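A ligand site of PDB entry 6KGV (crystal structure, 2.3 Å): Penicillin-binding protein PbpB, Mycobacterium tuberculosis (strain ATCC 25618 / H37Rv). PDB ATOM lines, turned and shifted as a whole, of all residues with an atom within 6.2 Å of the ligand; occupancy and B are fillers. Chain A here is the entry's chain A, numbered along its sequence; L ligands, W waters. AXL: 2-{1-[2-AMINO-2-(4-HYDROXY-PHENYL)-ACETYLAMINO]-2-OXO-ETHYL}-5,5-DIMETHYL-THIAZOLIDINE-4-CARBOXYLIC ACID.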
ATOM      1  N   PRO A 267      -3.200  -1.541   9.318  1.00  0.00           N
ATOM      2  CA  PRO A 267      -2.487  -2.815   9.509  1.00  0.00           C
ATOM      3  C   PRO A 267      -1.213  -2.663  10.303  1.00  0.00           C
ATOM      4  O   PRO A 267      -0.813  -3.604  11.009  1.00  0.00           O
ATOM      5  CB  PRO A 267      -2.219  -3.280   8.076  1.00  0.00           C
ATOM      6  CG  PRO A 267      -2.061  -1.962   7.303  1.00  0.00           C
ATOM      7  CD  PRO A 267      -3.045  -1.008   7.949  1.00  0.00           C
ATOM      8  N   GLY A 268      -0.561  -1.505  10.238  1.00  0.00           N
ATOM      9  CA  GLY A 268       0.755  -1.487  10.818  1.00  0.00           C
ATOM     10  C   GLY A 268       1.700  -2.363  10.015  1.00  0.00           C
ATOM     11  O   GLY A 268       1.523  -2.572   8.811  1.00  0.00           O
ATOM     12  N   SER A 269       2.675  -2.925  10.710  1.00  0.00           N
ATOM     13  CA  SER A 269       3.810  -3.581  10.074  1.00  0.00           C
ATOM     14  C   SER A 269       3.452  -4.819   9.284  1.00  0.00           C
ATOM     15  O   SER A 269       4.300  -5.274   8.500  1.00  0.00           O
ATOM     16  CB  SER A 269       4.838  -3.932  11.142  1.00  0.00           C
ATOM     17  OG  SER A 269       5.431  -2.762  11.602  1.00  0.00           O
ATOM     18  N   VAL A 270       2.257  -5.393   9.434  1.00  0.00           N
ATOM     19  CA  VAL A 270       1.940  -6.513   8.540  1.00  0.00           C
ATOM     20  C   VAL A 270       1.806  -6.034   7.114  1.00  0.00           C
ATOM     21  O   VAL A 270       1.898  -6.847   6.183  1.00  0.00           O
ATOM     22  CB  VAL A 270       0.664  -7.264   8.945  1.00  0.00           C
ATOM     23  CG1 VAL A 270       0.907  -8.028  10.216  1.00  0.00           C
ATOM     24  CG2 VAL A 270      -0.501  -6.276   9.089  1.00  0.00           C
ATOM     25  N   LYS A 272       4.065  -4.584   5.677  1.00  0.00           N
ATOM     26  CA  LYS A 272       5.402  -4.545   5.098  1.00  0.00           C
ATOM     27  C   LYS A 272       5.619  -5.624   4.059  1.00  0.00           C
ATOM     28  O   LYS A 272       6.636  -5.584   3.357  1.00  0.00           O
ATOM     29  CB  LYS A 272       6.452  -4.624   6.204  1.00  0.00           C
ATOM     30  CG  LYS A 272       6.536  -3.360   7.071  1.00  0.00           C
ATOM     31  CD  LYS A 272       7.564  -3.501   8.190  1.00  0.00           C
ATOM     32  CE  LYS A 272       7.737  -2.205   9.012  1.00  0.00           C
ATOM     33  NZ  LYS A 272       8.525  -2.415  10.270  1.00  0.00           N
ATOM     34  N   HIS A 305      10.900   6.609  13.464  1.00  0.00           N
ATOM     35  CA  HIS A 305      11.751   5.983  14.445  1.00  0.00           C
ATOM     36  C   HIS A 305      11.529   4.477  14.392  1.00  0.00           C
ATOM     37  O   HIS A 305      10.461   4.019  13.982  1.00  0.00           O
ATOM     38  CB  HIS A 305      11.399   6.534  15.845  1.00  0.00           C
ATOM     39  CG  HIS A 305      12.552   6.635  16.789  1.00  0.00           C
ATOM     40  ND1 HIS A 305      13.205   7.820  17.056  1.00  0.00           N
ATOM     41  CD2 HIS A 305      13.154   5.696  17.567  1.00  0.00           C
ATOM     42  CE1 HIS A 305      14.163   7.614  17.933  1.00  0.00           C
ATOM     43  NE2 HIS A 305      14.151   6.333  18.266  1.00  0.00           N
ATOM     44  N   ASP A 306      12.536   3.702  14.777  1.00  0.00           N
ATOM     45  CA  ASP A 306      12.313   2.291  15.013  1.00  0.00           C
ATOM     46  C   ASP A 306      11.857   2.070  16.456  1.00  0.00           C
ATOM     47  O   ASP A 306      12.103   2.884  17.342  1.00  0.00           O
ATOM     48  CB  ASP A 306      13.590   1.485  14.727  1.00  0.00           C
ATOM     49  CG  ASP A 306      13.787   1.199  13.222  1.00  0.00           C
ATOM     50  OD1 ASP A 306      12.879   1.492  12.421  1.00  0.00           O
ATOM     51  OD2 ASP A 306      14.852   0.660  12.858  1.00  0.00           O
ATOM     52  N   ALA A 307      11.177   0.939  16.692  1.00  0.00           N
ATOM     53  CA  ALA A 307      10.595   0.653  18.005  1.00  0.00           C
ATOM     54  C   ALA A 307      11.640   0.450  19.094  1.00  0.00           C
ATOM     55  O   ALA A 307      11.273   0.394  20.283  1.00  0.00           O
ATOM     56  CB  ALA A 307       9.697  -0.580  17.924  1.00  0.00           C
ATOM     57  N   TRP A 308      12.915   0.328  18.746  1.00  0.00           N
ATOM     58  CA  TRP A 308      14.000   0.239  19.706  1.00  0.00           C
ATOM     59  C   TRP A 308      15.057   1.252  19.317  1.00  0.00           C
ATOM     60  O   TRP A 308      15.255   1.513  18.126  1.00  0.00           O
ATOM     61  CB  TRP A 308      14.602  -1.189  19.782  1.00  0.00           C
ATOM     62  CG  TRP A 308      15.198  -1.723  18.482  1.00  0.00           C
ATOM     63  CD1 TRP A 308      16.528  -1.947  18.226  1.00  0.00           C
ATOM     64  CD2 TRP A 308      14.487  -2.134  17.302  1.00  0.00           C
ATOM     65  NE1 TRP A 308      16.687  -2.445  16.952  1.00  0.00           N
ATOM     66  CE2 TRP A 308      15.458  -2.579  16.364  1.00  0.00           C
ATOM     67  CE3 TRP A 308      13.134  -2.166  16.939  1.00  0.00           C
ATOM     68  CZ2 TRP A 308      15.107  -3.042  15.086  1.00  0.00           C
ATOM     69  CZ3 TRP A 308      12.788  -2.624  15.669  1.00  0.00           C
ATOM     70  CH2 TRP A 308      13.768  -3.052  14.755  1.00  0.00           C
ATOM     71  N   LYS A 323      13.100  -8.191  11.966  1.00  0.00           N
ATOM     72  CA  LYS A 323      13.072  -7.369  13.178  1.00  0.00           C
ATOM     73  C   LYS A 323      12.077  -6.219  13.095  1.00  0.00           C
ATOM     74  O   LYS A 323      11.857  -5.533  14.103  1.00  0.00           O
ATOM     75  CB  LYS A 323      14.466  -6.818  13.481  1.00  0.00           C
ATOM     76  CG  LYS A 323      15.484  -7.880  13.812  1.00  0.00           C
ATOM     77  CD  LYS A 323      16.783  -7.279  14.323  1.00  0.00           C
ATOM     78  CE  LYS A 323      17.797  -8.370  14.648  1.00  0.00           C
ATOM     79  NZ  LYS A 323      17.387  -9.250  15.783  1.00  0.00           N
ATOM     80  N   SER A 324      11.495  -6.011  11.921  1.00  0.00           N
ATOM     81  CA  SER A 324      10.492  -4.980  11.652  1.00  0.00           C
ATOM     82  C   SER A 324      11.044  -3.574  11.898  1.00  0.00           C
ATOM     83  O   SER A 324      10.480  -2.773  12.645  1.00  0.00           O
ATOM     84  CB  SER A 324       9.207  -5.242  12.429  1.00  0.00           C
ATOM     85  OG  SER A 324       8.092  -4.712  11.718  1.00  0.00           O
ATOM     86  N   SER A 325      12.144  -3.277  11.225  1.00  0.00           N
ATOM     87  CA  SER A 325      12.699  -1.922  11.194  1.00  0.00           C
ATOM     88  C   SER A 325      11.847  -1.054  10.257  1.00  0.00           C
ATOM     89  O   SER A 325      11.819  -1.298   9.048  1.00  0.00           O
ATOM     90  CB  SER A 325      14.149  -1.961  10.732  1.00  0.00           C
ATOM     91  OG  SER A 325      14.640  -0.659  10.461  1.00  0.00           O
ATOM     92  N   ASN A 326      11.132  -0.079  10.841  1.00  0.00           N
ATOM     93  CA  ASN A 326      10.407   0.916  10.051  1.00  0.00           C
ATOM     94  C   ASN A 326      11.366   1.698   9.167  1.00  0.00           C
ATOM     95  O   ASN A 326      11.115   1.915   7.977  1.00  0.00           O
ATOM     96  CB  ASN A 326       9.649   1.885  10.964  1.00  0.00           C
ATOM     97  CG  ASN A 326       8.444   1.249  11.663  1.00  0.00           C
ATOM     98  OD1 ASN A 326       7.973   0.183  11.284  1.00  0.00           O
ATOM     99  ND2 ASN A 326       7.938   1.936  12.675  1.00  0.00           N
ATOM    100  N   ILE A 382       4.906   1.313   6.119  1.00  0.00           N
ATOM    101  CA  ILE A 382       4.904   0.691   7.443  1.00  0.00           C
ATOM    102  C   ILE A 382       3.496   0.447   7.965  1.00  0.00           C
ATOM    103  O   ILE A 382       3.323   0.019   9.116  1.00  0.00           O
ATOM    104  CB  ILE A 382       5.730   1.492   8.462  1.00  0.00           C
ATOM    105  CG1 ILE A 382       5.065   2.847   8.757  1.00  0.00           C
ATOM    106  CG2 ILE A 382       7.209   1.589   8.006  1.00  0.00           C
ATOM    107  CD1 ILE A 382       5.887   3.735   9.655  1.00  0.00           C
ATOM    108  N   GLN A 384       0.600   2.550   8.195  1.00  0.00           N
ATOM    109  CA  GLN A 384      -0.249   3.577   8.776  1.00  0.00           C
ATOM    110  C   GLN A 384      -0.651   4.555   7.672  1.00  0.00           C
ATOM    111  O   GLN A 384       0.098   4.766   6.715  1.00  0.00           O
ATOM    112  CB  GLN A 384       0.454   4.302   9.962  1.00  0.00           C
ATOM    113  CG  GLN A 384       1.028   3.357  11.071  1.00  0.00           C
ATOM    114  CD  GLN A 384       0.160   3.226  12.362  1.00  0.00           C
ATOM    115  OE1 GLN A 384       0.696   3.002  13.454  1.00  0.00           O
ATOM    116  NE2 GLN A 384      -1.167   3.331  12.229  1.00  0.00           N
ATOM    117  N   THR A 461      10.706 -10.803  15.331  1.00  0.00           N
ATOM    118  CA  THR A 461       9.730 -10.259  16.267  1.00  0.00           C
ATOM    119  C   THR A 461       8.745 -11.307  16.792  1.00  0.00           C
ATOM    120  O   THR A 461       8.082 -11.056  17.789  1.00  0.00           O
ATOM    121  CB  THR A 461       8.953  -9.125  15.612  1.00  0.00           C
ATOM    122  OG1 THR A 461       8.367  -9.593  14.374  1.00  0.00           O
ATOM    123  CG2 THR A 461       9.870  -7.936  15.342  1.00  0.00           C
ATOM    124  N   LYS A 475       4.403 -12.435   9.633  1.00  0.00           N
ATOM    125  CA  LYS A 475       4.802 -11.071   9.950  1.00  0.00           C
ATOM    126  C   LYS A 475       3.906 -10.581  11.084  1.00  0.00           C
ATOM    127  O   LYS A 475       2.685 -10.797  11.057  1.00  0.00           O
ATOM    128  CB  LYS A 475       4.678 -10.150   8.729  1.00  0.00           C
ATOM    129  CG  LYS A 475       5.074  -8.697   8.979  1.00  0.00           C
ATOM    130  CD  LYS A 475       6.615  -8.584   9.179  1.00  0.00           C
ATOM    131  CE  LYS A 475       7.049  -7.187   9.616  1.00  0.00           C
ATOM    132  NZ  LYS A 475       6.779  -6.963  11.075  1.00  0.00           N
ATOM    133  N   THR A 476       4.538  -9.969  12.101  1.00  0.00           N
ATOM    134  CA  THR A 476       3.864  -9.312  13.215  1.00  0.00           C
ATOM    135  C   THR A 476       3.421  -7.904  12.808  1.00  0.00           C
ATOM    136  O   THR A 476       3.983  -7.300  11.885  1.00  0.00           O
ATOM    137  CB  THR A 476       4.778  -9.231  14.434  1.00  0.00           C
ATOM    138  OG1 THR A 476       6.075  -8.736  14.020  1.00  0.00           O
ATOM    139  CG2 THR A 476       4.953 -10.606  15.133  1.00  0.00           C
ATOM    140  N   GLY A 477       2.428  -7.375  13.515  1.00  0.00           N
ATOM    141  CA  GLY A 477       2.074  -5.970  13.379  1.00  0.00           C
ATOM    142  C   GLY A 477       1.660  -5.298  14.680  1.00  0.00           C
ATOM    143  O   GLY A 477       1.000  -5.908  15.527  1.00  0.00           O
ATOM    144  N   THR A 478       2.028  -4.028  14.842  1.00  0.00           N
ATOM    145  CA  THR A 478       1.561  -3.190  15.968  1.00  0.00           C
ATOM    146  C   THR A 478       1.235  -1.815  15.382  1.00  0.00           C
ATOM    147  O   THR A 478       2.137  -0.997  15.160  1.00  0.00           O
ATOM    148  CB  THR A 478       2.597  -3.057  17.092  1.00  0.00           C
ATOM    149  OG1 THR A 478       3.034  -4.354  17.531  1.00  0.00           O
ATOM    150  CG2 THR A 478       2.007  -2.341  18.302  1.00  0.00           C
ATOM    151  N   ALA A 479      -0.054  -1.559  15.155  1.00  0.00           N
ATOM    152  CA  ALA A 479      -0.508  -0.294  14.581  1.00  0.00           C
ATOM    153  C   ALA A 479      -1.154   0.568  15.658  1.00  0.00           C
ATOM    154  O   ALA A 479      -1.996   0.091  16.418  1.00  0.00           O
ATOM    155  CB  ALA A 479      -1.507  -0.540  13.444  1.00  0.00           C
ATOM    156  N   GLN A 480      -0.771   1.843  15.693  1.00  0.00           N
ATOM    157  CA  GLN A 480      -1.399   2.769  16.619  1.00  0.00           C
ATOM    158  C   GLN A 480      -2.797   3.141  16.122  1.00  0.00           C
ATOM    159  O   GLN A 480      -2.979   3.427  14.936  1.00  0.00           O
ATOM    160  CB  GLN A 480      -0.533   4.007  16.806  1.00  0.00           C
ATOM    161  CG  GLN A 480       0.794   3.705  17.493  1.00  0.00           C
ATOM    162  CD  GLN A 480       1.758   4.867  17.401  1.00  0.00           C
ATOM    163  OE1 GLN A 480       2.804   4.783  16.755  1.00  0.00           O
ATOM    164  NE2 GLN A 480       1.402   5.974  18.040  1.00  0.00           N
ATOM    165  N   ASP A 491      -0.902   6.804  21.844  1.00  0.00           N
ATOM    166  CA  ASP A 491       0.457   6.339  22.066  1.00  0.00           C
ATOM    167  C   ASP A 491       0.521   4.900  22.537  1.00  0.00           C
ATOM    168  O   ASP A 491       1.508   4.208  22.258  1.00  0.00           O
ATOM    169  CB  ASP A 491       1.178   7.232  23.077  1.00  0.00           C
ATOM    170  CG  ASP A 491       2.046   8.276  22.405  1.00  0.00           C
ATOM    171  OD1 ASP A 491       2.960   7.873  21.636  1.00  0.00           O
ATOM    172  OD2 ASP A 491       1.800   9.484  22.618  1.00  0.00           O
ATOM    173  N   TYR A 494      -3.259  -0.063  20.476  1.00  0.00           N
ATOM    174  CA  TYR A 494      -2.792  -0.691  19.247  1.00  0.00           C
ATOM    175  C   TYR A 494      -3.796  -1.689  18.681  1.00  0.00           C
ATOM    176  O   TYR A 494      -4.561  -2.315  19.420  1.00  0.00           O
ATOM    177  CB  TYR A 494      -1.463  -1.428  19.465  1.00  0.00           C
ATOM    178  CG  TYR A 494      -0.416  -0.601  20.162  1.00  0.00           C
ATOM    179  CD1 TYR A 494       0.197   0.466  19.513  1.00  0.00           C
ATOM    180  CD2 TYR A 494      -0.020  -0.896  21.459  1.00  0.00           C
ATOM    181  CE1 TYR A 494       1.183   1.227  20.143  1.00  0.00           C
ATOM    182  CE2 TYR A 494       0.965  -0.142  22.095  1.00  0.00           C
ATOM    183  CZ  TYR A 494       1.554   0.915  21.428  1.00  0.00           C
ATOM    184  OH  TYR A 494       2.517   1.672  22.064  1.00  0.00           O
HETATM  185  C1  AXL L   1       4.937  -2.058  12.622  1.00  0.00           C
HETATM  186  O1  AXL L   1       3.880  -2.459  13.105  1.00  0.00           O
HETATM  187  C2  AXL L   1       5.912  -1.215  13.433  1.00  0.00           C
HETATM  188  C3  AXL L   1       7.001  -2.189  13.881  1.00  0.00           C
HETATM  189  S4  AXL L   1       7.668  -1.825  15.472  1.00  0.00           S
HETATM  190  C5  AXL L   1       7.183  -3.345  16.252  1.00  0.00           C
HETATM  191  C51 AXL L   1       8.377  -4.299  16.316  1.00  0.00           C
HETATM  192  C52 AXL L   1       6.658  -3.091  17.674  1.00  0.00           C
HETATM  193  C6  AXL L   1       6.055  -3.881  15.379  1.00  0.00           C
HETATM  194  C61 AXL L   1       5.880  -5.370  15.461  1.00  0.00           C
HETATM  195  O62 AXL L   1       5.302  -5.847  16.456  1.00  0.00           O
HETATM  196  O63 AXL L   1       6.319  -6.063  14.516  1.00  0.00           O
HETATM  197  N7  AXL L   1       6.351  -3.476  14.026  1.00  0.00           N
HETATM  198  N8  AXL L   1       5.305  -0.537  14.568  1.00  0.00           N
HETATM  199  C9  AXL L   1       5.343   0.792  14.758  1.00  0.00           C
HETATM  200  O91 AXL L   1       6.041   1.539  14.091  1.00  0.00           O
HETATM  201  C10 AXL L   1       4.467   1.372  15.849  1.00  0.00           C
HETATM  202  N11 AXL L   1       4.387   2.817  15.748  1.00  0.00           N
HETATM  203  C12 AXL L   1       4.956   1.016  17.198  1.00  0.00           C
HETATM  204  C13 AXL L   1       4.177   0.216  18.001  1.00  0.00           C
HETATM  205  C14 AXL L   1       4.596  -0.144  19.280  1.00  0.00           C
HETATM  206  C15 AXL L   1       5.814   0.318  19.755  1.00  0.00           C
HETATM  207  C16 AXL L   1       6.613   1.131  18.957  1.00  0.00           C
HETATM  208  C17 AXL L   1       6.181   1.490  17.674  1.00  0.00           C
HETATM  209  O18 AXL L   1       6.224  -0.035  21.008  1.00  0.00           O
HETATM  210  O   HOH W   1      10.588  -0.528  14.195  1.00  0.00           O
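O1 of the ligand sits at hydrogen-bond distance from N of Thr 478.
O63 of the ligand lies within hydrogen-bond range of OG1 of Thr 476 (2.7 Å).
O1 of the ligand lies close to N of Ser 269, at 2.7 Å.
The side-chain amide oxygen (OE1) of Gln 480 lies within hydrogen-bond range of a nitrogen (N11) of the ligand (2.7 Å).
OG of Ser 324 sits at hydrogen-bond distance from N7 of the ligand, 3.1 Å away.
The side-chain hydroxyl (OG1) of Thr 478 lies within hydrogen-bond range of an oxygen (O62) of the ligand.
An oxygen (O91) of the ligand sits at hydrogen-bond distance from the side-chain amide nitrogen of Asn 326, 2.4 Å away.
O of Thr 478 is in hydrogen-bond range of N8 of the ligand, 3.3 Å away.
An oxygen (O63) of the ligand lies within salt-bridge range of the side-chain amino group of Lys 475 (3.6 Å).
C1 of the ligand is bonded to OG of Ser 269, at 1.3 Å.
The side-chain hydroxyl (OG) of Ser 324 is in hydrogen-bond range of the side-chain hydroxyl (OG) of Ser 269, at 3.3 Å.
NZ of Lys 272 lies within hydrogen-bond range of OG of Ser 269, at 3.4 Å.
The backbone carbonyl oxygen (O) of Asp 491 sits at hydrogen-bond distance from the side-chain hydroxyl (OH) of Tyr 494, at 2.7 Å.
OG1 of Thr 476 sits at hydrogen-bond distance from OG1 of Thr 461 (2.5 Å).
The backbone carbonyl oxygen (O) of Ile 382 is in hydrogen-bond range of the backbone NH (N) of Ser 269 (3.4 Å).
OG of Ser 324 is in hydrogen-bond range of NZ of Lys 272, at 2.7 Å.
The backbone NH (N) of Gln 480 lies within hydrogen-bond range of the side-chain amide oxygen (OE1) of Gln 384, at 2.9 Å.
OD1 of Asp 306 is in hydrogen-bond range of N of Asn 326 (2.8 Å).
Water W1 lies within hydrogen-bond range of the backbone carbonyl oxygen of Ser 324 (2.7 Å), the backbone NH of Ala 307 (3.0 Å), the backbone NH of Asn 326 (3.4 Å) and a sulfur (S4) of the ligand (3.4 Å).
C of Gly 268 touches O1 of the ligand (3.8 Å).
Lys 272 touches the ligand (NZ to C3, 3.9 Å).
CB of Ala 307 touches S4 of the ligand, at 3.4 Å.
C of Gly 477 touches O1 of the ligand, 3.9 Å away.
CE1 of Tyr 494 touches C14 of the ligand (3.8 Å).
Hydrophobic or aromatic side chains that line the ligand: Ala 307 and Tyr 494.
Of the 24 residues printed, 12 come within 4 Å of the ligand.
The nearest printed residue that does not touch the ligand is Thr 461 (4.1 Å).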
